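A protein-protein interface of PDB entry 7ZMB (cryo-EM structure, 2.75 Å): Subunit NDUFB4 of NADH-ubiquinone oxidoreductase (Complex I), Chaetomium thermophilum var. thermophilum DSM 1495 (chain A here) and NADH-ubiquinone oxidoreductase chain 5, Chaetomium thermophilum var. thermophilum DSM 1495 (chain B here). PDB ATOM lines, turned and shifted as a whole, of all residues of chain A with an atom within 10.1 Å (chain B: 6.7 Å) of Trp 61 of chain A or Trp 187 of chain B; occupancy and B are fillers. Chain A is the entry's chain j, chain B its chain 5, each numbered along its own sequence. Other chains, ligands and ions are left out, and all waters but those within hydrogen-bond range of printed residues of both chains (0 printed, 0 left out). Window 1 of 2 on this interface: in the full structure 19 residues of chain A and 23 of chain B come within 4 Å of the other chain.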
ATOM      1  N   LEU A  53      18.719  -7.720 -21.642  1.00  0.00           N
ATOM      2  CA  LEU A  53      18.506  -6.466 -20.933  1.00  0.00           C
ATOM      3  C   LEU A  53      19.028  -5.282 -21.730  1.00  0.00           C
ATOM      4  O   LEU A  53      18.402  -4.218 -21.747  1.00  0.00           O
ATOM      5  CB  LEU A  53      19.156  -6.525 -19.557  1.00  0.00           C
ATOM      6  CG  LEU A  53      18.240  -7.051 -18.455  1.00  0.00           C
ATOM      7  CD1 LEU A  53      18.889  -6.885 -17.094  1.00  0.00           C
ATOM      8  CD2 LEU A  53      16.910  -6.331 -18.513  1.00  0.00           C
ATOM      9  N   ALA A  54      20.172  -5.439 -22.396  1.00  0.00           N
ATOM     10  CA  ALA A  54      20.699  -4.350 -23.208  1.00  0.00           C
ATOM     11  C   ALA A  54      19.739  -3.994 -24.330  1.00  0.00           C
ATOM     12  O   ALA A  54      19.471  -2.813 -24.576  1.00  0.00           O
ATOM     13  CB  ALA A  54      22.072  -4.724 -23.764  1.00  0.00           C
ATOM     14  N   TYR A  55      19.209  -5.007 -25.012  1.00  0.00           N
ATOM     15  CA  TYR A  55      18.219  -4.777 -26.056  1.00  0.00           C
ATOM     16  C   TYR A  55      16.968  -4.120 -25.495  1.00  0.00           C
ATOM     17  O   TYR A  55      16.451  -3.153 -26.064  1.00  0.00           O
ATOM     18  CB  TYR A  55      17.878  -6.102 -26.740  1.00  0.00           C
ATOM     19  CG  TYR A  55      17.099  -5.947 -28.020  1.00  0.00           C
ATOM     20  CD1 TYR A  55      15.713  -5.864 -28.005  1.00  0.00           C
ATOM     21  CD2 TYR A  55      17.741  -5.906 -29.244  1.00  0.00           C
ATOM     22  CE1 TYR A  55      14.991  -5.729 -29.173  1.00  0.00           C
ATOM     23  CE2 TYR A  55      17.033  -5.771 -30.418  1.00  0.00           C
ATOM     24  CZ  TYR A  55      15.657  -5.683 -30.379  1.00  0.00           C
ATOM     25  OH  TYR A  55      14.946  -5.550 -31.549  1.00  0.00           O
ATOM     26  N   LYS A  56      16.476  -4.621 -24.363  1.00  0.00           N
ATOM     27  CA  LYS A  56      15.217  -4.136 -23.814  1.00  0.00           C
ATOM     28  C   LYS A  56      15.319  -2.748 -23.203  1.00  0.00           C
ATOM     29  O   LYS A  56      14.281  -2.135 -22.946  1.00  0.00           O
ATOM     30  CB  LYS A  56      14.691  -5.120 -22.773  1.00  0.00           C
ATOM     31  CG  LYS A  56      14.015  -6.341 -23.367  1.00  0.00           C
ATOM     32  CD  LYS A  56      12.853  -5.943 -24.264  1.00  0.00           C
ATOM     33  CE  LYS A  56      11.634  -5.552 -23.448  1.00  0.00           C
ATOM     34  NZ  LYS A  56      10.450  -5.295 -24.311  1.00  0.00           N
ATOM     35  N   THR A  57      16.516  -2.227 -22.968  1.00  0.00           N
ATOM     36  CA  THR A  57      16.674  -0.896 -22.388  1.00  0.00           C
ATOM     37  C   THR A  57      17.634  -0.062 -23.214  1.00  0.00           C
ATOM     38  O   THR A  57      18.526   0.601 -22.685  1.00  0.00           O
ATOM     39  CB  THR A  57      17.161  -0.966 -20.943  1.00  0.00           C
ATOM     40  OG1 THR A  57      18.396  -1.691 -20.885  1.00  0.00           O
ATOM     41  CG2 THR A  57      16.126  -1.648 -20.059  1.00  0.00           C
ATOM     42  N   ASP A  58      17.456  -0.068 -24.528  1.00  0.00           N
ATOM     43  CA  ASP A  58      18.343   0.639 -25.442  1.00  0.00           C
ATOM     44  C   ASP A  58      17.601   1.840 -26.015  1.00  0.00           C
ATOM     45  O   ASP A  58      16.517   1.691 -26.588  1.00  0.00           O
ATOM     46  CB  ASP A  58      18.834  -0.293 -26.546  1.00  0.00           C
ATOM     47  CG  ASP A  58      19.982   0.285 -27.322  1.00  0.00           C
ATOM     48  OD1 ASP A  58      20.312   1.465 -27.109  1.00  0.00           O
ATOM     49  OD2 ASP A  58      20.583  -0.447 -28.129  1.00  0.00           O
ATOM     50  N   GLY A  59      18.186   3.023 -25.855  1.00  0.00           N
ATOM     51  CA  GLY A  59      17.509   4.259 -26.153  1.00  0.00           C
ATOM     52  C   GLY A  59      16.495   4.684 -25.119  1.00  0.00           C
ATOM     53  O   GLY A  59      15.811   5.692 -25.324  1.00  0.00           O
ATOM     54  N   LEU A  60      16.381   3.955 -24.009  1.00  0.00           N
ATOM     55  CA  LEU A  60      15.279   4.181 -23.082  1.00  0.00           C
ATOM     56  C   LEU A  60      15.497   5.430 -22.239  1.00  0.00           C
ATOM     57  O   LEU A  60      14.543   6.151 -21.940  1.00  0.00           O
ATOM     58  CB  LEU A  60      15.092   2.949 -22.193  1.00  0.00           C
ATOM     59  CG  LEU A  60      14.135   3.017 -21.002  1.00  0.00           C
ATOM     60  CD1 LEU A  60      12.770   3.561 -21.407  1.00  0.00           C
ATOM     61  CD2 LEU A  60      14.006   1.648 -20.376  1.00  0.00           C
ATOM     62  N   TRP A  61      16.737   5.711 -21.853  1.00  0.00           N
ATOM     63  CA  TRP A  61      17.032   6.822 -20.964  1.00  0.00           C
ATOM     64  C   TRP A  61      18.025   7.792 -21.593  1.00  0.00           C
ATOM     65  O   TRP A  61      18.831   7.414 -22.444  1.00  0.00           O
ATOM     66  CB  TRP A  61      17.586   6.324 -19.638  1.00  0.00           C
ATOM     67  CG  TRP A  61      16.680   5.383 -18.943  1.00  0.00           C
ATOM     68  CD1 TRP A  61      15.373   5.585 -18.634  1.00  0.00           C
ATOM     69  CD2 TRP A  61      17.008   4.077 -18.466  1.00  0.00           C
ATOM     70  NE1 TRP A  61      14.865   4.489 -17.993  1.00  0.00           N
ATOM     71  CE2 TRP A  61      15.850   3.548 -17.877  1.00  0.00           C
ATOM     72  CE3 TRP A  61      18.172   3.309 -18.476  1.00  0.00           C
ATOM     73  CZ2 TRP A  61      15.820   2.287 -17.302  1.00  0.00           C
ATOM     74  CZ3 TRP A  61      18.142   2.060 -17.911  1.00  0.00           C
ATOM     75  CH2 TRP A  61      16.973   1.556 -17.331  1.00  0.00           C
ATOM     76  N   ASP A  62      17.949   9.050 -21.164  1.00  0.00           N
ATOM     77  CA  ASP A  62      18.903  10.077 -21.580  1.00  0.00           C
ATOM     78  C   ASP A  62      18.823  11.235 -20.601  1.00  0.00           C
ATOM     79  O   ASP A  62      17.753  11.819 -20.429  1.00  0.00           O
ATOM     80  CB  ASP A  62      18.617  10.557 -22.997  1.00  0.00           C
ATOM     81  CG  ASP A  62      19.429  11.780 -23.366  1.00  0.00           C
ATOM     82  OD1 ASP A  62      20.654  11.774 -23.119  1.00  0.00           O
ATOM     83  OD2 ASP A  62      18.848  12.747 -23.901  1.00  0.00           O
ATOM     84  N   LEU A  63      19.943  11.571 -19.968  1.00  0.00           N
ATOM     85  CA  LEU A  63      19.967  12.600 -18.938  1.00  0.00           C
ATOM     86  C   LEU A  63      20.309  13.980 -19.464  1.00  0.00           C
ATOM     87  O   LEU A  63      20.192  14.947 -18.707  1.00  0.00           O
ATOM     88  CB  LEU A  63      20.979  12.250 -17.847  1.00  0.00           C
ATOM     89  CG  LEU A  63      21.113  10.839 -17.300  1.00  0.00           C
ATOM     90  CD1 LEU A  63      22.055  10.856 -16.126  1.00  0.00           C
ATOM     91  CD2 LEU A  63      19.769  10.320 -16.880  1.00  0.00           C
ATOM     92  N   ARG A  64      20.664  14.098 -20.746  1.00  0.00           N
ATOM     93  CA  ARG A  64      21.569  15.141 -21.219  1.00  0.00           C
ATOM     94  C   ARG A  64      21.313  16.506 -20.600  1.00  0.00           C
ATOM     95  O   ARG A  64      22.209  17.102 -19.996  1.00  0.00           O
ATOM     96  CB  ARG A  64      21.506  15.251 -22.744  1.00  0.00           C
ATOM     97  CG  ARG A  64      22.605  16.144 -23.302  1.00  0.00           C
ATOM     98  CD  ARG A  64      23.932  15.414 -23.314  1.00  0.00           C
ATOM     99  NE  ARG A  64      25.075  16.321 -23.387  1.00  0.00           N
ATOM    100  CZ  ARG A  64      26.134  16.249 -22.590  1.00  0.00           C
ATOM    101  NH1 ARG A  64      27.125  17.107 -22.731  1.00  0.00           N
ATOM    102  NH2 ARG A  64      26.203  15.311 -21.661  1.00  0.00           N
ATOM    103  N   ALA A  65      20.108  17.036 -20.770  1.00  0.00           N
ATOM    104  CA  ALA A  65      19.771  18.326 -20.189  1.00  0.00           C
ATOM    105  C   ALA A  65      18.342  18.327 -19.678  1.00  0.00           C
ATOM    106  O   ALA A  65      17.651  19.349 -19.730  1.00  0.00           O
ATOM    107  CB  ALA A  65      19.986  19.455 -21.196  1.00  0.00           C
ATOM    108  N   LYS A  66      17.875  17.191 -19.177  1.00  0.00           N
ATOM    109  CA  LYS A  66      16.497  17.092 -18.714  1.00  0.00           C
ATOM    110  C   LYS A  66      16.337  17.905 -17.438  1.00  0.00           C
ATOM    111  O   LYS A  66      16.944  17.594 -16.409  1.00  0.00           O
ATOM    112  CB  LYS A  66      16.104  15.633 -18.498  1.00  0.00           C
ATOM    113  CG  LYS A  66      16.559  14.703 -19.598  1.00  0.00           C
ATOM    114  CD  LYS A  66      15.723  14.899 -20.842  1.00  0.00           C
ATOM    115  CE  LYS A  66      15.640  13.641 -21.675  1.00  0.00           C
ATOM    116  NZ  LYS A  66      15.186  12.469 -20.866  1.00  0.00           N
ATOM    117  N   ASP A  70      10.615  17.294 -16.451  1.00  0.00           N
ATOM    118  CA  ASP A  70      10.788  16.436 -17.611  1.00  0.00           C
ATOM    119  C   ASP A  70      11.317  15.083 -17.151  1.00  0.00           C
ATOM    120  O   ASP A  70      11.812  14.935 -16.033  1.00  0.00           O
ATOM    121  CB  ASP A  70      11.732  17.064 -18.645  1.00  0.00           C
ATOM    122  CG  ASP A  70      11.667  16.372 -19.997  1.00  0.00           C
ATOM    123  OD1 ASP A  70      11.350  15.165 -20.044  1.00  0.00           O
ATOM    124  OD2 ASP A  70      11.932  17.040 -21.018  1.00  0.00           O
ATOM    125  N   LEU A  71      11.207  14.095 -18.031  1.00  0.00           N
ATOM    126  CA  LEU A  71      11.509  12.717 -17.682  1.00  0.00           C
ATOM    127  C   LEU A  71      12.858  12.279 -18.241  1.00  0.00           C
ATOM    128  O   LEU A  71      13.267  12.687 -19.331  1.00  0.00           O
ATOM    129  CB  LEU A  71      10.414  11.782 -18.192  1.00  0.00           C
ATOM    130  CG  LEU A  71       8.979  12.237 -17.922  1.00  0.00           C
ATOM    131  CD1 LEU A  71       7.989  11.191 -18.401  1.00  0.00           C
ATOM    132  CD2 LEU A  71       8.773  12.537 -16.445  1.00  0.00           C
ATOM    133  N   ILE A  72      13.546  11.438 -17.469  1.00  0.00           N
ATOM    134  CA  ILE A  72      14.750  10.776 -17.959  1.00  0.00           C
ATOM    135  C   ILE A  72      14.429   9.892 -19.156  1.00  0.00           C
ATOM    136  O   ILE A  72      15.203   9.817 -20.118  1.00  0.00           O
ATOM    137  CB  ILE A  72      15.404   9.961 -16.828  1.00  0.00           C
ATOM    138  CG1 ILE A  72      15.865  10.872 -15.692  1.00  0.00           C
ATOM    139  CG2 ILE A  72      16.528   9.115 -17.367  1.00  0.00           C
ATOM    140  CD1 ILE A  72      16.666  10.160 -14.638  1.00  0.00           C
ATOM    141  N   SER A  73      13.297   9.195 -19.112  1.00  0.00           N
ATOM    142  CA  SER A  73      12.978   8.228 -20.150  1.00  0.00           C
ATOM    143  C   SER A  73      12.688   8.921 -21.472  1.00  0.00           C
ATOM    144  O   SER A  73      12.248  10.071 -21.516  1.00  0.00           O
ATOM    145  CB  SER A  73      11.781   7.376 -19.742  1.00  0.00           C
ATOM    146  OG  SER A  73      11.279   6.661 -20.854  1.00  0.00           O
ATOM    147  N   GLU A  74      12.954   8.205 -22.562  1.00  0.00           N
ATOM    148  CA  GLU A  74      12.657   8.689 -23.901  1.00  0.00           C
ATOM    149  C   GLU A  74      11.776   7.742 -24.700  1.00  0.00           C
ATOM    150  O   GLU A  74      11.390   8.082 -25.825  1.00  0.00           O
ATOM    151  CB  GLU A  74      13.952   8.949 -24.681  1.00  0.00           C
ATOM    152  CG  GLU A  74      14.695  10.206 -24.264  1.00  0.00           C
ATOM    153  CD  GLU A  74      15.873  10.509 -25.168  1.00  0.00           C
ATOM    154  OE1 GLU A  74      16.223   9.648 -26.002  1.00  0.00           O
ATOM    155  OE2 GLU A  74      16.441  11.615 -25.057  1.00  0.00           O
ATOM    156  N   ARG A  75      11.446   6.574 -24.163  1.00  0.00           N
ATOM    157  CA  ARG A  75      10.651   5.601 -24.896  1.00  0.00           C
ATOM    158  C   ARG A  75       9.697   4.869 -23.958  1.00  0.00           C
ATOM    159  O   ARG A  75       9.979   4.712 -22.772  1.00  0.00           O
ATOM    160  CB  ARG A  75      11.567   4.608 -25.618  1.00  0.00           C
ATOM    161  CG  ARG A  75      10.840   3.507 -26.366  1.00  0.00           C
ATOM    162  CD  ARG A  75      11.804   2.674 -27.196  1.00  0.00           C
ATOM    163  NE  ARG A  75      13.077   2.447 -26.517  1.00  0.00           N
ATOM    164  CZ  ARG A  75      13.248   1.605 -25.502  1.00  0.00           C
ATOM    165  NH1 ARG A  75      14.446   1.464 -24.952  1.00  0.00           N
ATOM    166  NH2 ARG A  75      12.225   0.901 -25.037  1.00  0.00           N
ATOM    167  OXT ARG A  75       8.620   4.426 -24.357  1.00  0.00           O
ATOM    168  N   PHE B  70      33.879  18.811 -22.551  1.00  0.00           N
ATOM    169  CA  PHE B  70      34.508  18.303 -21.335  1.00  0.00           C
ATOM    170  C   PHE B  70      35.860  18.976 -21.220  1.00  0.00           C
ATOM    171  O   PHE B  70      36.806  18.603 -21.917  1.00  0.00           O
ATOM    172  CB  PHE B  70      34.655  16.788 -21.370  1.00  0.00           C
ATOM    173  CG  PHE B  70      33.366  16.042 -21.195  1.00  0.00           C
ATOM    174  CD1 PHE B  70      32.167  16.707 -21.071  1.00  0.00           C
ATOM    175  CD2 PHE B  70      33.362  14.659 -21.151  1.00  0.00           C
ATOM    176  CE1 PHE B  70      30.988  16.016 -20.914  1.00  0.00           C
ATOM    177  CE2 PHE B  70      32.185  13.962 -20.995  1.00  0.00           C
ATOM    178  CZ  PHE B  70      31.000  14.643 -20.874  1.00  0.00           C
ATOM    179  N   MET B 182      29.974  10.463 -11.267  1.00  0.00           N
ATOM    180  CA  MET B 182      30.555  11.532 -12.069  1.00  0.00           C
ATOM    181  C   MET B 182      30.258  11.343 -13.550  1.00  0.00           C
ATOM    182  O   MET B 182      30.203  12.326 -14.294  1.00  0.00           O
ATOM    183  CB  MET B 182      32.060  11.623 -11.834  1.00  0.00           C
ATOM    184  CG  MET B 182      32.456  12.053 -10.443  1.00  0.00           C
ATOM    185  SD  MET B 182      34.245  12.212 -10.252  1.00  0.00           S
ATOM    186  CE  MET B 182      34.764  10.503 -10.206  1.00  0.00           C
ATOM    187  N   PHE B 183      30.067  10.098 -14.001  1.00  0.00           N
ATOM    188  CA  PHE B 183      29.568   9.877 -15.357  1.00  0.00           C
ATOM    189  C   PHE B 183      28.159  10.422 -15.519  1.00  0.00           C
ATOM    190  O   PHE B 183      27.816  10.943 -16.584  1.00  0.00           O
ATOM    191  CB  PHE B 183      29.572   8.396 -15.715  1.00  0.00           C
ATOM    192  CG  PHE B 183      30.930   7.815 -15.929  1.00  0.00           C
ATOM    193  CD1 PHE B 183      31.984   8.601 -16.327  1.00  0.00           C
ATOM    194  CD2 PHE B 183      31.144   6.468 -15.740  1.00  0.00           C
ATOM    195  CE1 PHE B 183      33.222   8.052 -16.529  1.00  0.00           C
ATOM    196  CE2 PHE B 183      32.384   5.922 -15.929  1.00  0.00           C
ATOM    197  CZ  PHE B 183      33.424   6.717 -16.321  1.00  0.00           C
ATOM    198  N   ALA B 184      27.328  10.291 -14.483  1.00  0.00           N
ATOM    199  CA  ALA B 184      25.997  10.881 -14.504  1.00  0.00           C
ATOM    200  C   ALA B 184      26.050  12.399 -14.461  1.00  0.00           C
ATOM    201  O   ALA B 184      25.187  13.061 -15.038  1.00  0.00           O
ATOM    202  CB  ALA B 184      25.172  10.344 -13.340  1.00  0.00           C
ATOM    203  N   ILE B 185      27.044  12.970 -13.781  1.00  0.00           N
ATOM    204  CA  ILE B 185      27.193  14.422 -13.778  1.00  0.00           C
ATOM    205  C   ILE B 185      27.631  14.915 -15.151  1.00  0.00           C
ATOM    206  O   ILE B 185      27.119  15.918 -15.655  1.00  0.00           O
ATOM    207  CB  ILE B 185      28.176  14.853 -12.678  1.00  0.00           C
ATOM    208  CG1 ILE B 185      27.607  14.541 -11.298  1.00  0.00           C
ATOM    209  CG2 ILE B 185      28.505  16.317 -12.803  1.00  0.00           C
ATOM    210  CD1 ILE B 185      28.400  15.148 -10.187  1.00  0.00           C
ATOM    211  N   LEU B 186      28.583  14.221 -15.774  1.00  0.00           N
ATOM    212  CA  LEU B 186      29.024  14.595 -17.116  1.00  0.00           C
ATOM    213  C   LEU B 186      27.912  14.412 -18.134  1.00  0.00           C
ATOM    214  O   LEU B 186      27.809  15.184 -19.091  1.00  0.00           O
ATOM    215  CB  LEU B 186      30.242  13.769 -17.524  1.00  0.00           C
ATOM    216  CG  LEU B 186      31.600  14.267 -17.050  1.00  0.00           C
ATOM    217  CD1 LEU B 186      32.698  13.374 -17.586  1.00  0.00           C
ATOM    218  CD2 LEU B 186      31.811  15.697 -17.486  1.00  0.00           C
ATOM    219  N   TRP B 187      27.083  13.384 -17.954  1.00  0.00           N
ATOM    220  CA  TRP B 187      26.015  13.115 -18.906  1.00  0.00           C
ATOM    221  C   TRP B 187      24.932  14.180 -18.834  1.00  0.00           C
ATOM    222  O   TRP B 187      24.477  14.683 -19.865  1.00  0.00           O
ATOM    223  CB  TRP B 187      25.426  11.727 -18.649  1.00  0.00           C
ATOM    224  CG  TRP B 187      24.512  11.233 -19.724  1.00  0.00           C
ATOM    225  CD1 TRP B 187      24.179  11.874 -20.877  1.00  0.00           C
ATOM    226  CD2 TRP B 187      23.801   9.996 -19.738  1.00  0.00           C
ATOM    227  NE1 TRP B 187      23.311  11.115 -21.608  1.00  0.00           N
ATOM    228  CE2 TRP B 187      23.062   9.954 -20.930  1.00  0.00           C
ATOM    229  CE3 TRP B 187      23.722   8.915 -18.859  1.00  0.00           C
ATOM    230  CZ2 TRP B 187      22.256   8.877 -21.266  1.00  0.00           C
ATOM    231  CZ3 TRP B 187      22.923   7.852 -19.197  1.00  0.00           C
ATOM    232  CH2 TRP B 187      22.201   7.838 -20.385  1.00  0.00           C
ATOM    233  N   SER B 188      24.513  14.544 -17.628  1.00  0.00           N
ATOM    234  CA  SER B 188      23.338  15.385 -17.457  1.00  0.00           C
ATOM    235  C   SER B 188      23.642  16.875 -17.422  1.00  0.00           C
ATOM    236  O   SER B 188      22.701  17.675 -17.445  1.00  0.00           O
ATOM    237  CB  SER B 188      22.600  14.994 -16.179  1.00  0.00           C
ATOM    238  OG  SER B 188      23.263  15.499 -15.041  1.00  0.00           O
ATOM    239  N   LEU B 189      24.923  17.272 -17.423  1.00  0.00           N
ATOM    240  CA  LEU B 189      25.269  18.720 -17.311  1.00  0.00           C
ATOM    241  C   LEU B 189      26.332  19.121 -18.336  1.00  0.00           C
ATOM    242  O   LEU B 189      26.460  20.321 -18.601  1.00  0.00           O
ATOM    243  CB  LEU B 189      25.728  19.057 -15.890  1.00  0.00           C
ATOM    244  CG  LEU B 189      24.677  19.708 -14.993  1.00  0.00           C
ATOM    245  CD1 LEU B 189      23.688  20.509 -15.821  1.00  0.00           C
ATOM    246  CD2 LEU B 189      23.947  18.668 -14.160  1.00  0.00           C
ATOM    247  N   GLY B 190      27.093  18.159 -18.850  1.00  0.00           N
ATOM    248  CA  GLY B 190      28.125  18.440 -19.861  1.00  0.00           C
ATOM    249  C   GLY B 190      29.459  18.784 -19.242  1.00  0.00           C
ATOM    250  O   GLY B 190      30.414  18.973 -19.995  1.00  0.00           O
ATOM    251  N   ASN B 191      29.508  18.920 -17.923  1.00  0.00           N
ATOM    252  CA  ASN B 191      30.800  19.154 -17.227  1.00  0.00           C
ATOM    253  C   ASN B 191      30.648  18.758 -15.764  1.00  0.00           C
ATOM    254  O   ASN B 191      29.575  18.276 -15.395  1.00  0.00           O
ATOM    255  CB  ASN B 191      31.347  20.577 -17.385  1.00  0.00           C
ATOM    256  CG  ASN B 191      32.843  20.616 -17.605  1.00  0.00           C
ATOM    257  OD1 ASN B 191      33.362  19.962 -18.506  1.00  0.00           O
ATOM    258  ND2 ASN B 191      33.544  21.387 -16.793  1.00  0.00           N
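Among the printed residues, pairs that only touch across the chains: Arg 64 of chain A with Gly 190 of chain B (3.3 Å), Leu 63 of chain A with Ser 188 of chain B (3.4 Å), Leu 63 of chain A with Trp 187 of chain B (3.6 Å), Arg 64 of chain A with Leu 189 of chain B (3.7 Å), Trp 61 of chain A with Trp 187 of chain B (3.9 Å) and Leu 63 of chain A with Ala 184 of chain B (3.98 Å).
Of the 11 printed residues of chain B, 6 touch a printed residue of chain A. Hydrophobic or aromatic side chains of chain B that line the printed part of chain A: Trp 187. Printed residues of chain A that touch a printed residue of chain B: Trp 61, Asp 62, Leu 63 and Arg 64.
The indole nitrogen (NE1) of Trp 187 of chain B lies within hydrogen-bond range of the side-chain carboxylate (OD1) of Asp 62 of chain A (3.1 Å). The guanidinium group (NH2) of Arg 64 of chain A lies within hydrogen-bond range of the backbone carbonyl oxygen (O) of Leu 186 of chain B, at 3.0 Å. NH2 of Arg 64 of chain A is in hydrogen-bond range of O of Trp 187 of chain B (2.6 Å). O of Ser 188 of chain B sits close to O of Arg 64 of chain A (2.7 Å).
The backbone NH (N) of Arg 64 of chain A lies within hydrogen-bond range of the side-chain carboxylate (OD1) of Asp 62 of chain A, at 3.3 Å. NZ of Lys 66 of chain A sits at hydrogen-bond distance from O of Asp 62 of chain A (2.7 Å). The backbone NH (N) of Asp 62 of chain A sits at hydrogen-bond distance from the backbone carbonyl oxygen (O) of Ile 72 of chain A (3.0 Å). The side-chain hydroxyl of Ser 188 of chain B sits at hydrogen-bond distance from the backbone carbonyl oxygen of Ala 184 of chain B (3.1 Å).
Lys 56 of chain A touches none of the printed residues of chain B. Of the printed residues of chain B, Trp 61 of chain A touches Trp 187. Of the printed residues of chain B, Asp 62 of chain A touches Trp 187 (3.1 Å). Of the printed residues of chain B, Leu 63 of chain A touches Ala 184 (3.98 Å), Trp 187 (3.6 Å) and Ser 188 (3.4 Å). Printed residues of chain B within 4 Å of Arg 64 of chain A: Leu 186, Trp 187, Ser 188, Leu 189 and Gly 190. Trp 187 of chain B touches four residues of chain A. Ser 188 of chain B touches two residues of chain A. Printed residues of chain A within 4 Å of Leu 189 of chain B: Arg 64 (3.7 Å). The nearest printed residue of chain B that does not touch Trp 61 of chain A is Ser 188 of chain B (10.1 Å). The nearest printed residue of chain A that does not touch Leu 189 of chain B is Leu 63 of chain A (5.4 Å).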
